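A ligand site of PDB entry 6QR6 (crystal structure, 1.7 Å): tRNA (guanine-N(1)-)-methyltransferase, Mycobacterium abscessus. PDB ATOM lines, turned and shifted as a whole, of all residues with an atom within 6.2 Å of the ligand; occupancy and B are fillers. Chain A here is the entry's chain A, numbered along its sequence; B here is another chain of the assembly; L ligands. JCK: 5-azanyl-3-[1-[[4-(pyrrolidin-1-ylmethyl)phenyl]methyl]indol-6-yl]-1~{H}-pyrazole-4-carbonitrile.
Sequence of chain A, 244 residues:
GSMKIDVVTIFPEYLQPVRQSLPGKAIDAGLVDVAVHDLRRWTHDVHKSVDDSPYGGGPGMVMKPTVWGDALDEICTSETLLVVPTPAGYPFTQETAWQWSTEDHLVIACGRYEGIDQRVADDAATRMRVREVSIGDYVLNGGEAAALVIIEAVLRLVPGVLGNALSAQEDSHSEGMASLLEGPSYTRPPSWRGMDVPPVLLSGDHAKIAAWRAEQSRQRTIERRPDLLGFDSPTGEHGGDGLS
The backbone carbonyl oxygen (O) of Val 133 sits close to a nitrogen (N30) of the ligand, at 3.4 Å.
O of Pro 85 touches C10 of the ligand (3.3 Å).
CD of Pro 87 touches C06 of the ligand, at 3.5 Å.
O of Gly 111 touches C12 of the ligand, at 3.4 Å.
C of Arg 112 touches C13 of the ligand, 3.7 Å away.
Tyr 113 touches the ligand (O to C13, 3.3 Å).
Glu 114 touches the ligand.
N of Ile 135 touches N30 of the ligand, 3.5 Å away.
CA of Val 139 touches N03 of the ligand, at 3.7 Å.
O of Asn 141 touches C15 of the ligand, 3.4 Å away.
Gly 142 touches the ligand.
N of Gly 143 touches C10 of the ligand, at 3.5 Å.
Ala 146 touches the ligand.
NH2 of Arg 156 of chain B touches C27 of the ligand, 3.9 Å away.
CG of Glu 182 of chain B touches C22 of the ligand, 3.4 Å away.
Hydrophobic or aromatic side chains that line the ligand: Pro 85, Pro 87, Ile 135, Tyr 138, Val 139, Leu 140 and Ala 146.
The backbone carbonyl oxygen (O) of Ile 135 is in hydrogen-bond range of the side-chain hydroxyl (OH) of Tyr 138, 3.2 Å away.
The backbone carbonyl oxygen of Gly 136 lies within hydrogen-bond range of the side-chain hydroxyl of Ser 134 (3.2 Å).
O of Gly 111 sits at hydrogen-bond distance from N of Gly 143 (2.9 Å).
O of Val 133 sits at hydrogen-bond distance from N of Thr 86, 2.9 Å away.
The backbone carbonyl oxygen (O) of Val 84 lies within hydrogen-bond range of the backbone NH (N) of Val 133 (3.1 Å).
The side-chain amide oxygen (OD1) of Asn 141 lies within hydrogen-bond range of the guanidinium group (NE) of Arg 156 of chain B, 3.2 Å away.
The guanidinium group (NE) of Arg 112 lies within salt-bridge range of the side-chain carboxylate (OE1) of Glu 144 (2.7 Å).
The backbone carbonyl oxygen (O) of Tyr 138 is in hydrogen-bond range of a nitrogen (N03) of the ligand, 2.7 Å away.
A nitrogen (N01) of the ligand lies within hydrogen-bond range of the backbone carbonyl oxygen of Gly 136.
The backbone NH (N) of Leu 140 lies within hydrogen-bond range of a nitrogen (N04) of the ligand (3.0 Å).
A nitrogen (N01) of the ligand lies within hydrogen-bond range of the side-chain hydroxyl (OG) of Ser 134 (3.0 Å).
The backbone NH (N) of Thr 86 lies within hydrogen-bond range of a nitrogen (N30) of the ligand (3.5 Å).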
ATOM      1  N   VAL A  84     -13.182  17.016   4.228  1.00  0.00           N
ATOM      2  CA  VAL A  84     -14.402  17.747   4.520  1.00  0.00           C
ATOM      3  C   VAL A  84     -15.615  16.853   4.263  1.00  0.00           C
ATOM      4  O   VAL A  84     -16.006  16.665   3.117  1.00  0.00           O
ATOM      5  CB  VAL A  84     -14.548  19.023   3.658  1.00  0.00           C
ATOM      6  CG1 VAL A  84     -15.756  19.844   4.101  1.00  0.00           C
ATOM      7  CG2 VAL A  84     -13.272  19.865   3.727  1.00  0.00           C
ATOM      8  N   PRO A  85     -16.178  16.261   5.327  1.00  0.00           N
ATOM      9  CA  PRO A  85     -17.423  15.497   5.127  1.00  0.00           C
ATOM     10  C   PRO A  85     -18.537  16.382   4.575  1.00  0.00           C
ATOM     11  O   PRO A  85     -18.663  17.522   4.982  1.00  0.00           O
ATOM     12  CB  PRO A  85     -17.760  14.997   6.540  1.00  0.00           C
ATOM     13  CG  PRO A  85     -16.394  14.929   7.244  1.00  0.00           C
ATOM     14  CD  PRO A  85     -15.664  16.150   6.694  1.00  0.00           C
ATOM     15  N   THR A  86     -19.330  15.832   3.663  1.00  0.00           N
ATOM     16  CA  THR A  86     -20.461  16.567   3.078  1.00  0.00           C
ATOM     17  C   THR A  86     -21.375  15.567   2.380  1.00  0.00           C
ATOM     18  O   THR A  86     -20.890  14.632   1.765  1.00  0.00           O
ATOM     19  CB  THR A  86     -20.015  17.660   2.084  1.00  0.00           C
ATOM     20  OG1 THR A  86     -21.124  18.053   1.240  1.00  0.00           O
ATOM     21  CG2 THR A  86     -18.855  17.208   1.232  1.00  0.00           C
ATOM     22  N   PRO A  87     -22.690  15.789   2.474  1.00  0.00           N
ATOM     23  CA  PRO A  87     -23.595  14.891   1.762  1.00  0.00           C
ATOM     24  C   PRO A  87     -23.385  14.964   0.236  1.00  0.00           C
ATOM     25  O   PRO A  87     -23.832  14.067  -0.491  1.00  0.00           O
ATOM     26  CB  PRO A  87     -24.992  15.373   2.182  1.00  0.00           C
ATOM     27  CG  PRO A  87     -24.804  16.736   2.705  1.00  0.00           C
ATOM     28  CD  PRO A  87     -23.386  16.851   3.205  1.00  0.00           C
ATOM     29  N   CYS A 110     -15.408  19.378  10.351  1.00  0.00           N
ATOM     30  CA  CYS A 110     -16.804  18.970  10.540  1.00  0.00           C
ATOM     31  C   CYS A 110     -17.779  20.137  10.476  1.00  0.00           C
ATOM     32  O   CYS A 110     -17.764  20.991  11.360  1.00  0.00           O
ATOM     33  CB  CYS A 110     -16.974  18.281  11.892  1.00  0.00           C
ATOM     34  SG  CYS A 110     -15.999  16.802  12.039  1.00  0.00           S
ATOM     35  N   GLY A 111     -18.657  20.141   9.474  1.00  0.00           N
ATOM     36  CA  GLY A 111     -19.680  21.162   9.383  1.00  0.00           C
ATOM     37  C   GLY A 111     -20.939  20.798  10.162  1.00  0.00           C
ATOM     38  O   GLY A 111     -21.124  19.655  10.586  1.00  0.00           O
ATOM     39  N   ARG A 112     -21.786  21.807  10.335  1.00  0.00           N
ATOM     40  CA  ARG A 112     -23.147  21.653  10.851  1.00  0.00           C
ATOM     41  C   ARG A 112     -24.042  22.573  10.039  1.00  0.00           C
ATOM     42  O   ARG A 112     -23.587  23.160   9.064  1.00  0.00           O
ATOM     43  CB  ARG A 112     -23.212  21.975  12.344  1.00  0.00           C
ATOM     44  CG  ARG A 112     -22.677  20.868  13.253  1.00  0.00           C
ATOM     45  CD  ARG A 112     -23.814  19.946  13.698  1.00  0.00           C
ATOM     46  NE  ARG A 112     -23.324  18.620  14.047  1.00  0.00           N
ATOM     47  CZ  ARG A 112     -24.079  17.683  14.629  1.00  0.00           C
ATOM     48  NH1 ARG A 112     -25.331  17.965  14.946  1.00  0.00           N
ATOM     49  NH2 ARG A 112     -23.560  16.492  14.913  1.00  0.00           N
ATOM     50  N   TYR A 113     -25.316  22.691  10.412  1.00  0.00           N
ATOM     51  CA  TYR A 113     -26.286  23.489   9.653  1.00  0.00           C
ATOM     52  C   TYR A 113     -26.344  23.011   8.192  1.00  0.00           C
ATOM     53  O   TYR A 113     -26.429  21.809   7.951  1.00  0.00           O
ATOM     54  CB  TYR A 113     -25.945  24.986   9.757  1.00  0.00           C
ATOM     55  CG  TYR A 113     -25.733  25.473  11.178  1.00  0.00           C
ATOM     56  CD1 TYR A 113     -26.809  25.860  11.966  1.00  0.00           C
ATOM     57  CD2 TYR A 113     -24.460  25.534  11.734  1.00  0.00           C
ATOM     58  CE1 TYR A 113     -26.626  26.294  13.265  1.00  0.00           C
ATOM     59  CE2 TYR A 113     -24.270  25.963  13.029  1.00  0.00           C
ATOM     60  CZ  TYR A 113     -25.357  26.348  13.792  1.00  0.00           C
ATOM     61  OH  TYR A 113     -25.152  26.781  15.088  1.00  0.00           O
ATOM     62  N   GLU A 114     -26.285  23.906   7.216  1.00  0.00           N
ATOM     63  CA  GLU A 114     -26.343  23.469   5.821  1.00  0.00           C
ATOM     64  C   GLU A 114     -24.965  23.179   5.244  1.00  0.00           C
ATOM     65  O   GLU A 114     -24.841  22.778   4.099  1.00  0.00           O
ATOM     66  CB  GLU A 114     -27.051  24.493   4.937  1.00  0.00           C
ATOM     67  CG  GLU A 114     -28.518  24.683   5.275  1.00  0.00           C
ATOM     68  CD  GLU A 114     -29.320  23.409   5.114  1.00  0.00           C
ATOM     69  OE1 GLU A 114     -29.661  22.774   6.134  1.00  0.00           O
ATOM     70  OE2 GLU A 114     -29.598  23.026   3.956  1.00  0.00           O
ATOM     71  N   GLY A 115     -23.920  23.363   6.050  1.00  0.00           N
ATOM     72  CA  GLY A 115     -22.559  23.145   5.575  1.00  0.00           C
ATOM     73  C   GLY A 115     -21.686  24.375   5.701  1.00  0.00           C
ATOM     74  O   GLY A 115     -22.073  25.348   6.337  1.00  0.00           O
ATOM     75  N   ILE A 116     -20.515  24.325   5.087  1.00  0.00           N
ATOM     76  CA  ILE A 116     -19.522  25.403   5.195  1.00  0.00           C
ATOM     77  C   ILE A 116     -19.488  26.194   3.912  1.00  0.00           C
ATOM     78  O   ILE A 116     -19.557  25.612   2.833  1.00  0.00           O
ATOM     79  CB  ILE A 116     -18.121  24.820   5.478  1.00  0.00           C
ATOM     80  CG1 ILE A 116     -18.174  23.896   6.704  1.00  0.00           C
ATOM     81  CG2 ILE A 116     -17.084  25.930   5.656  1.00  0.00           C
ATOM     82  CD1 ILE A 116     -16.877  23.126   6.958  1.00  0.00           C
ATOM     83  N   VAL A 133     -15.906  14.507   0.909  1.00  0.00           N
ATOM     84  CA  VAL A 133     -16.331  13.104   0.803  1.00  0.00           C
ATOM     85  C   VAL A 133     -17.608  12.860   1.571  1.00  0.00           C
ATOM     86  O   VAL A 133     -17.932  13.585   2.506  1.00  0.00           O
ATOM     87  CB  VAL A 133     -15.233  12.121   1.348  1.00  0.00           C
ATOM     88  CG1 VAL A 133     -13.974  12.202   0.502  1.00  0.00           C
ATOM     89  CG2 VAL A 133     -14.892  12.422   2.812  1.00  0.00           C
ATOM     90  N   SER A 134     -18.327  11.811   1.170  1.00  0.00           N
ATOM     91  CA  SER A 134     -19.525  11.359   1.858  1.00  0.00           C
ATOM     92  C   SER A 134     -19.416   9.900   2.246  1.00  0.00           C
ATOM     93  O   SER A 134     -18.962   9.096   1.430  1.00  0.00           O
ATOM     94  CB  SER A 134     -20.741  11.553   0.963  1.00  0.00           C
ATOM     95  OG  SER A 134     -21.867  10.881   1.513  1.00  0.00           O
ATOM     96  N   ILE A 135     -19.846   9.547   3.461  1.00  0.00           N
ATOM     97  CA  ILE A 135     -19.749   8.150   3.919  1.00  0.00           C
ATOM     98  C   ILE A 135     -20.930   7.264   3.529  1.00  0.00           C
ATOM     99  O   ILE A 135     -20.893   6.051   3.741  1.00  0.00           O
ATOM    100  CB  ILE A 135     -19.550   8.056   5.453  1.00  0.00           C
ATOM    101  CG1 ILE A 135     -20.721   8.701   6.223  1.00  0.00           C
ATOM    102  CG2 ILE A 135     -18.207   8.692   5.839  1.00  0.00           C
ATOM    103  CD1 ILE A 135     -20.842   8.186   7.686  1.00  0.00           C
ATOM    104  N   GLY A 136     -21.963   7.843   2.937  1.00  0.00           N
ATOM    105  CA  GLY A 136     -23.073   7.007   2.517  1.00  0.00           C
ATOM    106  C   GLY A 136     -24.269   7.781   2.013  1.00  0.00           C
ATOM    107  O   GLY A 136     -24.335   8.994   2.136  1.00  0.00           O
ATOM    108  N   ASP A 137     -25.247   7.062   1.459  1.00  0.00           N
ATOM    109  CA  ASP A 137     -26.375   7.768   0.829  1.00  0.00           C
ATOM    110  C   ASP A 137     -27.540   7.965   1.770  1.00  0.00           C
ATOM    111  O   ASP A 137     -28.620   7.424   1.560  1.00  0.00           O
ATOM    112  CB  ASP A 137     -26.814   7.022  -0.431  1.00  0.00           C
ATOM    113  CG  ASP A 137     -25.802   7.147  -1.551  1.00  0.00           C
ATOM    114  OD1 ASP A 137     -25.101   8.183  -1.578  1.00  0.00           O
ATOM    115  OD2 ASP A 137     -25.702   6.240  -2.381  1.00  0.00           O
ATOM    116  N   TYR A 138     -27.300   8.754   2.814  1.00  0.00           N
ATOM    117  CA  TYR A 138     -28.289   9.087   3.817  1.00  0.00           C
ATOM    118  C   TYR A 138     -27.853  10.455   4.304  1.00  0.00           C
ATOM    119  O   TYR A 138     -26.726  10.861   4.044  1.00  0.00           O
ATOM    120  CB  TYR A 138     -28.326   8.079   4.981  1.00  0.00           C
ATOM    121  CG  TYR A 138     -26.945   7.538   5.309  1.00  0.00           C
ATOM    122  CD1 TYR A 138     -26.020   8.299   6.031  1.00  0.00           C
ATOM    123  CD2 TYR A 138     -26.552   6.289   4.843  1.00  0.00           C
ATOM    124  CE1 TYR A 138     -24.760   7.810   6.292  1.00  0.00           C
ATOM    125  CE2 TYR A 138     -25.297   5.787   5.108  1.00  0.00           C
ATOM    126  CZ  TYR A 138     -24.395   6.555   5.825  1.00  0.00           C
ATOM    127  OH  TYR A 138     -23.140   6.030   6.060  1.00  0.00           O
ATOM    128  N   VAL A 139     -28.737  11.130   5.040  1.00  0.00           N
ATOM    129  CA  VAL A 139     -28.458  12.495   5.497  1.00  0.00           C
ATOM    130  C   VAL A 139     -28.241  12.540   6.995  1.00  0.00           C
ATOM    131  O   VAL A 139     -29.055  12.021   7.770  1.00  0.00           O
ATOM    132  CB  VAL A 139     -29.600  13.451   5.108  1.00  0.00           C
ATOM    133  CG1 VAL A 139     -29.289  14.870   5.577  1.00  0.00           C
ATOM    134  CG2 VAL A 139     -29.828  13.392   3.601  1.00  0.00           C
ATOM    135  N   LEU A 140     -27.126  13.135   7.426  1.00  0.00           N
ATOM    136  CA  LEU A 140     -26.808  13.284   8.844  1.00  0.00           C
ATOM    137  C   LEU A 140     -27.043  14.725   9.289  1.00  0.00           C
ATOM    138  O   LEU A 140     -27.400  15.568   8.463  1.00  0.00           O
ATOM    139  CB  LEU A 140     -25.344  12.891   9.112  1.00  0.00           C
ATOM    140  CG  LEU A 140     -24.921  11.482   8.678  1.00  0.00           C
ATOM    141  CD1 LEU A 140     -23.413  11.328   8.795  1.00  0.00           C
ATOM    142  CD2 LEU A 140     -25.623  10.425   9.529  1.00  0.00           C
ATOM    143  N   ASN A 141     -26.835  15.005  10.574  1.00  0.00           N
ATOM    144  CA  ASN A 141     -26.981  16.376  11.087  1.00  0.00           C
ATOM    145  C   ASN A 141     -25.727  17.226  10.892  1.00  0.00           C
ATOM    146  O   ASN A 141     -25.775  18.460  11.004  1.00  0.00           O
ATOM    147  CB  ASN A 141     -27.321  16.382  12.579  1.00  0.00           C
ATOM    148  CG  ASN A 141     -28.732  15.936  12.864  1.00  0.00           C
ATOM    149  OD1 ASN A 141     -29.659  16.212  12.110  1.00  0.00           O
ATOM    150  ND2 ASN A 141     -28.896  15.219  13.974  1.00  0.00           N
ATOM    151  N   GLY A 142     -24.607  16.575  10.638  1.00  0.00           N
ATOM    152  CA  GLY A 142     -23.345  17.285  10.514  1.00  0.00           C
ATOM    153  C   GLY A 142     -22.234  16.296  10.265  1.00  0.00           C
ATOM    154  O   GLY A 142     -22.497  15.098  10.136  1.00  0.00           O
ATOM    155  N   GLY A 143     -20.999  16.793  10.212  1.00  0.00           N
ATOM    156  CA  GLY A 143     -19.860  15.958   9.850  1.00  0.00           C
ATOM    157  C   GLY A 143     -19.274  15.055  10.928  1.00  0.00           C
ATOM    158  O   GLY A 143     -18.447  14.202  10.609  1.00  0.00           O
ATOM    159  N   GLU A 144     -19.698  15.216  12.179  1.00  0.00           N
ATOM    160  CA  GLU A 144     -19.044  14.504  13.279  1.00  0.00           C
ATOM    161  C   GLU A 144     -19.177  12.979  13.191  1.00  0.00           C
ATOM    162  O   GLU A 144     -18.209  12.253  13.374  1.00  0.00           O
ATOM    163  CB  GLU A 144     -19.579  14.995  14.613  1.00  0.00           C
ATOM    164  CG  GLU A 144     -19.138  16.418  14.991  1.00  0.00           C
ATOM    165  CD  GLU A 144     -19.953  17.519  14.328  1.00  0.00           C
ATOM    166  OE1 GLU A 144     -20.976  17.245  13.653  1.00  0.00           O
ATOM    167  OE2 GLU A 144     -19.560  18.696  14.508  1.00  0.00           O
ATOM    168  N   ALA A 146     -19.596  11.299  10.569  1.00  0.00           N
ATOM    169  CA  ALA A 146     -18.806  10.901   9.421  1.00  0.00           C
ATOM    170  C   ALA A 146     -17.332  10.863   9.807  1.00  0.00           C
ATOM    171  O   ALA A 146     -16.604   9.978   9.373  1.00  0.00           O
ATOM    172  CB  ALA A 146     -19.029  11.844   8.226  1.00  0.00           C
ATOM    173  N   ILE A 150     -14.768   7.728   9.357  1.00  0.00           N
ATOM    174  CA  ILE A 150     -13.525   7.883   8.614  1.00  0.00           C
ATOM    175  C   ILE A 150     -12.301   7.561   9.478  1.00  0.00           C
ATOM    176  O   ILE A 150     -11.408   6.828   9.032  1.00  0.00           O
ATOM    177  CB  ILE A 150     -13.417   9.311   8.042  1.00  0.00           C
ATOM    178  CG1 ILE A 150     -14.467   9.492   6.932  1.00  0.00           C
ATOM    179  CG2 ILE A 150     -12.006   9.552   7.487  1.00  0.00           C
ATOM    180  CD1 ILE A 150     -14.694  10.962   6.534  1.00  0.00           C
ATOM    181  N   ARG B 156     -33.597  12.191  12.895  1.00  0.00           N
ATOM    182  CA  ARG B 156     -33.911  13.514  12.348  1.00  0.00           C
ATOM    183  C   ARG B 156     -35.159  13.477  11.451  1.00  0.00           C
ATOM    184  O   ARG B 156     -35.659  14.525  11.038  1.00  0.00           O
ATOM    185  CB  ARG B 156     -32.698  14.087  11.612  1.00  0.00           C
ATOM    186  CG  ARG B 156     -32.193  13.241  10.480  1.00  0.00           C
ATOM    187  CD  ARG B 156     -30.866  13.765   9.960  1.00  0.00           C
ATOM    188  NE  ARG B 156     -30.945  15.113   9.404  1.00  0.00           N
ATOM    189  CZ  ARG B 156     -31.508  15.414   8.238  1.00  0.00           C
ATOM    190  NH1 ARG B 156     -32.091  14.482   7.482  1.00  0.00           N
ATOM    191  NH2 ARG B 156     -31.501  16.679   7.814  1.00  0.00           N
ATOM    192  N   LEU B 180     -30.288  14.168  -6.462  1.00  0.00           N
ATOM    193  CA  LEU B 180     -29.198  15.014  -6.933  1.00  0.00           C
ATOM    194  C   LEU B 180     -28.358  15.467  -5.736  1.00  0.00           C
ATOM    195  O   LEU B 180     -28.865  15.522  -4.617  1.00  0.00           O
ATOM    196  CB  LEU B 180     -29.727  16.240  -7.684  1.00  0.00           C
ATOM    197  CG  LEU B 180     -30.075  16.156  -9.165  1.00  0.00           C
ATOM    198  CD1 LEU B 180     -30.573  17.505  -9.644  1.00  0.00           C
ATOM    199  CD2 LEU B 180     -28.871  15.725  -9.993  1.00  0.00           C
ATOM    200  N   GLU B 182     -26.400  18.275  -3.498  1.00  0.00           N
ATOM    201  CA  GLU B 182     -26.545  19.700  -3.218  1.00  0.00           C
ATOM    202  C   GLU B 182     -25.378  20.493  -3.781  1.00  0.00           C
ATOM    203  O   GLU B 182     -24.229  20.041  -3.746  1.00  0.00           O
ATOM    204  CB  GLU B 182     -26.673  19.939  -1.719  1.00  0.00           C
ATOM    205  CG  GLU B 182     -28.098  20.043  -1.236  1.00  0.00           C
ATOM    206  CD  GLU B 182     -28.751  21.360  -1.618  1.00  0.00           C
ATOM    207  OE1 GLU B 182     -28.135  22.424  -1.398  1.00  0.00           O
ATOM    208  OE2 GLU B 182     -29.888  21.332  -2.146  1.00  0.00           O
HETATM  209  C10 JCK L   1     -21.483  17.143   6.747  1.00  0.00           C
HETATM  210  C13 JCK L   1     -23.954  19.646   7.797  1.00  0.00           C
HETATM  211  C15 JCK L   1     -26.125  18.483   7.616  1.00  0.00           C
HETATM  212  C17 JCK L   1     -26.412  19.465   5.220  1.00  0.00           C
HETATM  213  C20 JCK L   1     -29.507  19.493   2.894  1.00  0.00           C
HETATM  214  C22 JCK L   1     -30.271  18.899   1.160  1.00  0.00           C
HETATM  215  C24 JCK L   1     -29.527  16.624   1.182  1.00  0.00           C
HETATM  216  C26 JCK L   1     -29.082  18.582   5.196  1.00  0.00           C
HETATM  217  C28 JCK L   1     -22.672  13.005   5.244  1.00  0.00           C
HETATM  218  N01 JCK L   1     -23.161  10.779   4.244  1.00  0.00           N
HETATM  219  C02 JCK L   1     -23.541  12.019   4.837  1.00  0.00           C
HETATM  220  N03 JCK L   1     -24.801  12.429   5.099  1.00  0.00           N
HETATM  221  N04 JCK L   1     -24.737  13.672   5.666  1.00  0.00           N
HETATM  222  C05 JCK L   1     -23.482  14.026   5.805  1.00  0.00           C
HETATM  223  C06 JCK L   1     -23.095  15.402   6.337  1.00  0.00           C
HETATM  224  C07 JCK L   1     -24.143  16.233   6.666  1.00  0.00           C
HETATM  225  C08 JCK L   1     -23.851  17.553   7.090  1.00  0.00           C
HETATM  226  C09 JCK L   1     -22.547  17.994   7.128  1.00  0.00           C
HETATM  227  C11 JCK L   1     -21.773  15.841   6.335  1.00  0.00           C
HETATM  228  C12 JCK L   1     -22.617  19.340   7.568  1.00  0.00           C
HETATM  229  N14 JCK L   1     -24.672  18.584   7.499  1.00  0.00           N
HETATM  230  C16 JCK L   1     -26.946  18.790   6.309  1.00  0.00           C
HETATM  231  C18 JCK L   1     -27.235  19.706   4.101  1.00  0.00           C
HETATM  232  C19 JCK L   1     -28.559  19.248   4.089  1.00  0.00           C
HETATM  233  N21 JCK L   1     -29.283  18.860   1.896  1.00  0.00           N
HETATM  234  C23 JCK L   1     -30.287  17.549   0.377  1.00  0.00           C
HETATM  235  C25 JCK L   1     -28.943  17.331   2.121  1.00  0.00           C
HETATM  236  C27 JCK L   1     -28.279  18.343   6.293  1.00  0.00           C
HETATM  237  C29 JCK L   1     -21.165  12.882   5.123  1.00  0.00           C
HETATM  238  N30 JCK L   1     -20.069  12.714   5.008  1.00  0.00           N
